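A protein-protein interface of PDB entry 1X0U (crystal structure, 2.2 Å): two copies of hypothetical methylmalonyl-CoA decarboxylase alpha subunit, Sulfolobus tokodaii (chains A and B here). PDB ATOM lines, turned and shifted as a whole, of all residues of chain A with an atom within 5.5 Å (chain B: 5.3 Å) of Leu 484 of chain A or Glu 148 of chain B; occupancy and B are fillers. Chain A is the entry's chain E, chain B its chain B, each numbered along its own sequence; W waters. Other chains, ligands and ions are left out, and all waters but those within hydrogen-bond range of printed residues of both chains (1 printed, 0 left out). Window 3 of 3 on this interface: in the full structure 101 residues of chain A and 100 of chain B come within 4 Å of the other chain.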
ATOM      1  N   HIS A 414     -27.301 -13.639  13.902  1.00  0.00           N
ATOM      2  CA  HIS A 414     -26.786 -13.330  15.233  1.00  0.00           C
ATOM      3  C   HIS A 414     -27.900 -12.655  16.031  1.00  0.00           C
ATOM      4  O   HIS A 414     -28.205 -13.036  17.167  1.00  0.00           O
ATOM      5  CB  HIS A 414     -25.593 -12.376  15.123  1.00  0.00           C
ATOM      6  CG  HIS A 414     -25.172 -11.772  16.429  1.00  0.00           C
ATOM      7  ND1 HIS A 414     -25.399 -10.449  16.744  1.00  0.00           N
ATOM      8  CD2 HIS A 414     -24.520 -12.305  17.491  1.00  0.00           C
ATOM      9  CE1 HIS A 414     -24.901 -10.191  17.939  1.00  0.00           C
ATOM     10  NE2 HIS A 414     -24.364 -11.300  18.415  1.00  0.00           N
ATOM     11  N   ILE A 415     -28.514 -11.658  15.411  1.00  0.00           N
ATOM     12  CA  ILE A 415     -29.588 -10.890  16.032  1.00  0.00           C
ATOM     13  C   ILE A 415     -30.828 -11.726  16.337  1.00  0.00           C
ATOM     14  O   ILE A 415     -31.415 -11.607  17.417  1.00  0.00           O
ATOM     15  CB  ILE A 415     -30.006  -9.698  15.124  1.00  0.00           C
ATOM     16  CG1 ILE A 415     -28.777  -8.855  14.780  1.00  0.00           C
ATOM     17  CG2 ILE A 415     -31.025  -8.811  15.845  1.00  0.00           C
ATOM     18  CD1 ILE A 415     -29.001  -7.906  13.634  1.00  0.00           C
ATOM     19  N   ILE A 419     -30.347 -10.889  21.122  1.00  0.00           N
ATOM     20  CA  ILE A 419     -29.251 -10.070  21.624  1.00  0.00           C
ATOM     21  C   ILE A 419     -29.827  -9.010  22.578  1.00  0.00           C
ATOM     22  O   ILE A 419     -31.041  -8.774  22.589  1.00  0.00           O
ATOM     23  CB  ILE A 419     -28.484  -9.409  20.456  1.00  0.00           C
ATOM     24  CG1 ILE A 419     -29.377  -8.409  19.710  1.00  0.00           C
ATOM     25  CG2 ILE A 419     -28.009 -10.494  19.498  1.00  0.00           C
ATOM     26  CD1 ILE A 419     -28.619  -7.575  18.656  1.00  0.00           C
ATOM     27  N   LYS A 420     -28.980  -8.385  23.387  1.00  0.00           N
ATOM     28  CA  LYS A 420     -29.476  -7.397  24.343  1.00  0.00           C
ATOM     29  C   LYS A 420     -30.445  -6.366  23.776  1.00  0.00           C
ATOM     30  O   LYS A 420     -31.534  -6.175  24.315  1.00  0.00           O
ATOM     31  CB  LYS A 420     -28.318  -6.683  25.033  1.00  0.00           C
ATOM     32  CG  LYS A 420     -27.584  -7.549  26.042  1.00  0.00           C
ATOM     33  CD  LYS A 420     -26.521  -6.741  26.774  1.00  0.00           C
ATOM     34  CE  LYS A 420     -25.839  -7.566  27.852  1.00  0.00           C
ATOM     35  NZ  LYS A 420     -25.007  -6.696  28.736  1.00  0.00           N
ATOM     36  N   SER A 421     -30.066  -5.709  22.686  1.00  0.00           N
ATOM     37  CA  SER A 421     -30.936  -4.697  22.102  1.00  0.00           C
ATOM     38  C   SER A 421     -32.270  -5.278  21.666  1.00  0.00           C
ATOM     39  O   SER A 421     -33.209  -4.538  21.398  1.00  0.00           O
ATOM     40  CB  SER A 421     -30.255  -4.031  20.912  1.00  0.00           C
ATOM     41  OG  SER A 421     -29.930  -4.998  19.926  1.00  0.00           O
ATOM     42  N   LEU A 422     -32.359  -6.604  21.595  1.00  0.00           N
ATOM     43  CA  LEU A 422     -33.608  -7.251  21.194  1.00  0.00           C
ATOM     44  C   LEU A 422     -34.413  -7.781  22.397  1.00  0.00           C
ATOM     45  O   LEU A 422     -35.524  -8.285  22.231  1.00  0.00           O
ATOM     46  CB  LEU A 422     -33.322  -8.400  20.223  1.00  0.00           C
ATOM     47  CG  LEU A 422     -34.506  -8.882  19.372  1.00  0.00           C
ATOM     48  CD1 LEU A 422     -34.751  -7.890  18.249  1.00  0.00           C
ATOM     49  CD2 LEU A 422     -34.217 -10.252  18.796  1.00  0.00           C
ATOM     50  N   VAL A 427     -26.437 -12.319  28.340  1.00  0.00           N
ATOM     51  CA  VAL A 427     -25.766 -12.860  27.176  1.00  0.00           C
ATOM     52  C   VAL A 427     -24.391 -13.330  27.606  1.00  0.00           C
ATOM     53  O   VAL A 427     -23.597 -12.544  28.116  1.00  0.00           O
ATOM     54  CB  VAL A 427     -25.596 -11.791  26.073  1.00  0.00           C
ATOM     55  CG1 VAL A 427     -24.682 -12.322  24.955  1.00  0.00           C
ATOM     56  CG2 VAL A 427     -26.958 -11.409  25.505  1.00  0.00           C
ATOM     57  N   TRP A 478     -14.219  -8.762  21.898  1.00  0.00           N
ATOM     58  CA  TRP A 478     -14.519  -7.450  21.344  1.00  0.00           C
ATOM     59  C   TRP A 478     -15.915  -7.051  21.804  1.00  0.00           C
ATOM     60  O   TRP A 478     -16.120  -5.965  22.353  1.00  0.00           O
ATOM     61  CB  TRP A 478     -14.495  -7.486  19.819  1.00  0.00           C
ATOM     62  CG  TRP A 478     -14.570  -6.124  19.192  1.00  0.00           C
ATOM     63  CD1 TRP A 478     -13.522  -5.289  18.914  1.00  0.00           C
ATOM     64  CD2 TRP A 478     -15.755  -5.438  18.766  1.00  0.00           C
ATOM     65  NE1 TRP A 478     -13.982  -4.128  18.335  1.00  0.00           N
ATOM     66  CE2 TRP A 478     -15.347  -4.192  18.234  1.00  0.00           C
ATOM     67  CE3 TRP A 478     -17.121  -5.753  18.784  1.00  0.00           C
ATOM     68  CZ2 TRP A 478     -16.261  -3.262  17.719  1.00  0.00           C
ATOM     69  CZ3 TRP A 478     -18.032  -4.824  18.273  1.00  0.00           C
ATOM     70  CH2 TRP A 478     -17.594  -3.595  17.748  1.00  0.00           C
ATOM     71  N   ALA A 479     -16.872  -7.939  21.564  1.00  0.00           N
ATOM     72  CA  ALA A 479     -18.255  -7.702  21.951  1.00  0.00           C
ATOM     73  C   ALA A 479     -18.342  -7.433  23.454  1.00  0.00           C
ATOM     74  O   ALA A 479     -18.998  -6.487  23.878  1.00  0.00           O
ATOM     75  CB  ALA A 479     -19.114  -8.902  21.577  1.00  0.00           C
ATOM     76  N   ALA A 480     -17.674  -8.259  24.255  1.00  0.00           N
ATOM     77  CA  ALA A 480     -17.692  -8.070  25.703  1.00  0.00           C
ATOM     78  C   ALA A 480     -17.100  -6.709  26.101  1.00  0.00           C
ATOM     79  O   ALA A 480     -17.531  -6.105  27.091  1.00  0.00           O
ATOM     80  CB  ALA A 480     -16.928  -9.193  26.399  1.00  0.00           C
ATOM     81  N   LYS A 482     -17.463  -4.082  24.498  1.00  0.00           N
ATOM     82  CA  LYS A 482     -18.486  -3.108  24.133  1.00  0.00           C
ATOM     83  C   LYS A 482     -19.747  -3.337  24.956  1.00  0.00           C
ATOM     84  O   LYS A 482     -20.786  -2.738  24.686  1.00  0.00           O
ATOM     85  CB  LYS A 482     -18.826  -3.226  22.641  1.00  0.00           C
ATOM     86  CG  LYS A 482     -17.613  -3.203  21.719  1.00  0.00           C
ATOM     87  CD  LYS A 482     -16.755  -1.979  21.998  1.00  0.00           C
ATOM     88  CE  LYS A 482     -15.600  -1.866  21.010  1.00  0.00           C
ATOM     89  NZ  LYS A 482     -14.722  -0.702  21.330  1.00  0.00           N
ATOM     90  N   GLY A 483     -19.651  -4.215  25.950  1.00  0.00           N
ATOM     91  CA  GLY A 483     -20.796  -4.510  26.798  1.00  0.00           C
ATOM     92  C   GLY A 483     -21.902  -5.346  26.162  1.00  0.00           C
ATOM     93  O   GLY A 483     -22.931  -5.563  26.784  1.00  0.00           O
ATOM     94  N   LEU A 484     -21.698  -5.840  24.944  1.00  0.00           N
ATOM     95  CA  LEU A 484     -22.731  -6.629  24.274  1.00  0.00           C
ATOM     96  C   LEU A 484     -22.960  -8.018  24.883  1.00  0.00           C
ATOM     97  O   LEU A 484     -24.051  -8.585  24.767  1.00  0.00           O
ATOM     98  CB  LEU A 484     -22.415  -6.745  22.779  1.00  0.00           C
ATOM     99  CG  LEU A 484     -22.217  -5.381  22.107  1.00  0.00           C
ATOM    100  CD1 LEU A 484     -22.040  -5.548  20.603  1.00  0.00           C
ATOM    101  CD2 LEU A 484     -23.425  -4.493  22.407  1.00  0.00           C
ATOM    102  N   VAL A 485     -21.933  -8.581  25.507  1.00  0.00           N
ATOM    103  CA  VAL A 485     -22.081  -9.873  26.157  1.00  0.00           C
ATOM    104  C   VAL A 485     -21.647  -9.615  27.589  1.00  0.00           C
ATOM    105  O   VAL A 485     -20.626  -8.981  27.839  1.00  0.00           O
ATOM    106  CB  VAL A 485     -21.211 -11.001  25.513  1.00  0.00           C
ATOM    107  CG1 VAL A 485     -20.800 -10.619  24.108  1.00  0.00           C
ATOM    108  CG2 VAL A 485     -20.020 -11.331  26.387  1.00  0.00           C
ATOM    109  N   ASP A 486     -22.440 -10.083  28.533  1.00  0.00           N
ATOM    110  CA  ASP A 486     -22.124  -9.839  29.924  1.00  0.00           C
ATOM    111  C   ASP A 486     -20.857 -10.494  30.408  1.00  0.00           C
ATOM    112  O   ASP A 486     -20.164  -9.935  31.259  1.00  0.00           O
ATOM    113  CB  ASP A 486     -23.309 -10.246  30.788  1.00  0.00           C
ATOM    114  CG  ASP A 486     -24.512  -9.379  30.530  1.00  0.00           C
ATOM    115  OD1 ASP A 486     -24.400  -8.159  30.760  1.00  0.00           O
ATOM    116  OD2 ASP A 486     -25.558  -9.904  30.096  1.00  0.00           O
ATOM    117  N   ALA B 144     -19.935  -5.861  15.402  1.00  0.00           N
ATOM    118  CA  ALA B 144     -21.100  -6.297  16.172  1.00  0.00           C
ATOM    119  C   ALA B 144     -21.973  -5.158  16.708  1.00  0.00           C
ATOM    120  O   ALA B 144     -23.146  -5.366  17.012  1.00  0.00           O
ATOM    121  CB  ALA B 144     -20.639  -7.192  17.334  1.00  0.00           C
ATOM    122  N   LEU B 145     -21.392  -3.970  16.845  1.00  0.00           N
ATOM    123  CA  LEU B 145     -22.122  -2.809  17.325  1.00  0.00           C
ATOM    124  C   LEU B 145     -23.193  -2.443  16.310  1.00  0.00           C
ATOM    125  O   LEU B 145     -24.247  -1.935  16.665  1.00  0.00           O
ATOM    126  CB  LEU B 145     -21.159  -1.627  17.515  1.00  0.00           C
ATOM    127  CG  LEU B 145     -20.807  -1.123  18.924  1.00  0.00           C
ATOM    128  CD1 LEU B 145     -21.152  -2.136  19.998  1.00  0.00           C
ATOM    129  CD2 LEU B 145     -19.328  -0.786  18.957  1.00  0.00           C
ATOM    130  N   SER B 146     -22.921  -2.686  15.034  1.00  0.00           N
ATOM    131  CA  SER B 146     -23.898  -2.356  14.008  1.00  0.00           C
ATOM    132  C   SER B 146     -25.081  -3.331  14.088  1.00  0.00           C
ATOM    133  O   SER B 146     -26.234  -2.953  13.874  1.00  0.00           O
ATOM    134  CB  SER B 146     -23.241  -2.404  12.633  1.00  0.00           C
ATOM    135  OG  SER B 146     -24.168  -2.048  11.625  1.00  0.00           O
ATOM    136  N   LEU B 147     -24.797  -4.589  14.411  1.00  0.00           N
ATOM    137  CA  LEU B 147     -25.862  -5.573  14.531  1.00  0.00           C
ATOM    138  C   LEU B 147     -26.700  -5.215  15.759  1.00  0.00           C
ATOM    139  O   LEU B 147     -27.924  -5.303  15.719  1.00  0.00           O
ATOM    140  CB  LEU B 147     -25.286  -6.983  14.666  1.00  0.00           C
ATOM    141  CG  LEU B 147     -24.419  -7.457  13.492  1.00  0.00           C
ATOM    142  CD1 LEU B 147     -23.890  -8.864  13.782  1.00  0.00           C
ATOM    143  CD2 LEU B 147     -25.239  -7.438  12.199  1.00  0.00           C
ATOM    144  N   GLU B 148     -26.037  -4.798  16.839  1.00  0.00           N
ATOM    145  CA  GLU B 148     -26.742  -4.401  18.061  1.00  0.00           C
ATOM    146  C   GLU B 148     -27.698  -3.263  17.695  1.00  0.00           C
ATOM    147  O   GLU B 148     -28.827  -3.193  18.200  1.00  0.00           O
ATOM    148  CB  GLU B 148     -25.750  -3.916  19.123  1.00  0.00           C
ATOM    149  CG  GLU B 148     -26.342  -3.748  20.536  1.00  0.00           C
ATOM    150  CD  GLU B 148     -26.671  -5.085  21.205  1.00  0.00           C
ATOM    151  OE1 GLU B 148     -26.033  -6.105  20.866  1.00  0.00           O
ATOM    152  OE2 GLU B 148     -27.559  -5.117  22.083  1.00  0.00           O
ATOM    153  N   GLY B 149     -27.238  -2.375  16.810  1.00  0.00           N
ATOM    154  CA  GLY B 149     -28.065  -1.265  16.370  1.00  0.00           C
ATOM    155  C   GLY B 149     -29.329  -1.755  15.685  1.00  0.00           C
ATOM    156  O   GLY B 149     -30.413  -1.194  15.865  1.00  0.00           O
ATOM    157  N   TYR B 150     -29.187  -2.806  14.884  1.00  0.00           N
ATOM    158  CA  TYR B 150     -30.319  -3.407  14.185  1.00  0.00           C
ATOM    159  C   TYR B 150     -31.327  -4.005  15.184  1.00  0.00           C
ATOM    160  O   TYR B 150     -32.546  -3.878  15.010  1.00  0.00           O
ATOM    161  CB  TYR B 150     -29.824  -4.500  13.222  1.00  0.00           C
ATOM    162  CG  TYR B 150     -29.591  -4.012  11.806  1.00  0.00           C
ATOM    163  CD1 TYR B 150     -28.363  -4.190  11.178  1.00  0.00           C
ATOM    164  CD2 TYR B 150     -30.595  -3.343  11.107  1.00  0.00           C
ATOM    165  CE1 TYR B 150     -28.132  -3.705   9.885  1.00  0.00           C
ATOM    166  CE2 TYR B 150     -30.381  -2.858   9.816  1.00  0.00           C
ATOM    167  CZ  TYR B 150     -29.146  -3.039   9.212  1.00  0.00           C
ATOM    168  OH  TYR B 150     -28.918  -2.527   7.949  1.00  0.00           O
ATOM    169  N   GLY B 151     -30.810  -4.657  16.224  1.00  0.00           N
ATOM    170  CA  GLY B 151     -31.678  -5.229  17.238  1.00  0.00           C
ATOM    171  C   GLY B 151     -32.545  -4.145  17.859  1.00  0.00           C
ATOM    172  O   GLY B 151     -33.744  -4.338  18.061  1.00  0.00           O
ATOM    173  N   ALA B 152     -31.943  -2.990  18.135  1.00  0.00           N
ATOM    174  CA  ALA B 152     -32.673  -1.879  18.738  1.00  0.00           C
ATOM    175  C   ALA B 152     -33.804  -1.370  17.836  1.00  0.00           C
ATOM    176  O   ALA B 152     -34.910  -1.135  18.305  1.00  0.00           O
ATOM    177  CB  ALA B 152     -31.709  -0.748  19.083  1.00  0.00           C
HETATM  178  O   HOH W   1     -26.103  -8.082  22.850  1.00  0.00           O
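Of the printed residues of chain B, Ile 419 of chain A touches Leu 147 and Glu 148.
Printed residues of chain B within 4 Å of Leu 422 of chain A: Gly 151.
Of the printed residues of chain B, Trp 478 of chain A touches Ala 144 (3.6 Å) and Leu 145 (3.5 Å).
Of chain B, only Ala 144, Leu 145 and Glu 148 come within 4 Å of Leu 484 of chain A.
Val 485 of chain A touches none of the printed residues of chain B.
Printed residues of chain A within 4 Å of Gly 151 of chain B: Ile 415, Ser 421 and Leu 422.
Of the printed residues of chain A, Ala 152 of chain B touches Ser 421 (3.4 Å).
The nearest residue of chain A that does not touch Glu 148 of chain B is Leu 422 of chain A (5.0 Å).
The nearest printed residue of chain A that does not touch Leu 145 of chain B is Ala 479 of chain A (6.2 Å).
Water W1 lies within hydrogen-bond range of the side-chain carboxylate (OE1) of Glu 148 of chain B, the backbone carbonyl oxygen (O) of Leu 484 of chain A and the backbone NH (N) of Lys 420 of chain A.
Hydrophobic or aromatic side chains of chain A within 4 Å of the printed part of chain B: His 414, Ile 415, Ile 419, Leu 422, Trp 478 and Leu 484.
Among the printed residues, 17 pairs touch across the chains.
No position is printed for both chains.
Of the 17 pairs that touch across the chains among the printed residues, none has its exchanged pair printed and touching as well.
The backbone NH of Ala 152 of chain B is in hydrogen-bond range of the side-chain hydroxyl of Ser 421 of chain A (3.4 Å).
The backbone NH (N) of Ser 421 of chain A is in hydrogen-bond range of the side-chain carboxylate (OE2) of Glu 148 of chain B, 2.6 Å away.
The backbone carbonyl oxygen (O) of Ser 421 of chain A lies close to the backbone carbonyl oxygen (O) of Gly 151 of chain B (3.4 Å).
O of Ala 479 of chain A lies within hydrogen-bond range of N of Leu 484 of chain A (3.0 Å).
The side-chain amino group (NZ) of Lys 420 of chain A is in salt-bridge range of the side-chain carboxylate (OD1) of Asp 486 of chain A (2.6 Å).
The side-chain amino group (NZ) of Lys 420 of chain A lies within hydrogen-bond range of the backbone carbonyl oxygen (O) of Gly 483 of chain A (3.1 Å).
Among the printed residues, merely in contact across the chains: His 414 of chain A with Leu 147 of chain B (3.7 Å), Ile 415 of chain A with Leu 147 of chain B (3.5 Å), Ile 415 of chain A with Tyr 150 of chain B (3.5 Å), Ile 415 of chain A with Gly 151 of chain B (3.9 Å), Ile 419 of chain A with Leu 147 of chain B (3.8 Å), Ile 419 of chain A with Glu 148 of chain B (3.7 Å), Lys 420 of chain A with Glu 148 of chain B (3.4 Å), Leu 422 of chain A with Gly 151 of chain B (3.7 Å), Trp 478 of chain A with Ala 144 of chain B (3.6 Å), Trp 478 of chain A with Leu 145 of chain B (3.5 Å), Lys 482 of chain A with Leu 145 of chain B (3.7 Å), Leu 484 of chain A with Ala 144 of chain B (3.8 Å), Leu 484 of chain A with Leu 145 of chain B (3.6 Å) and Leu 484 of chain A with Glu 148 of chain B (3.4 Å).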
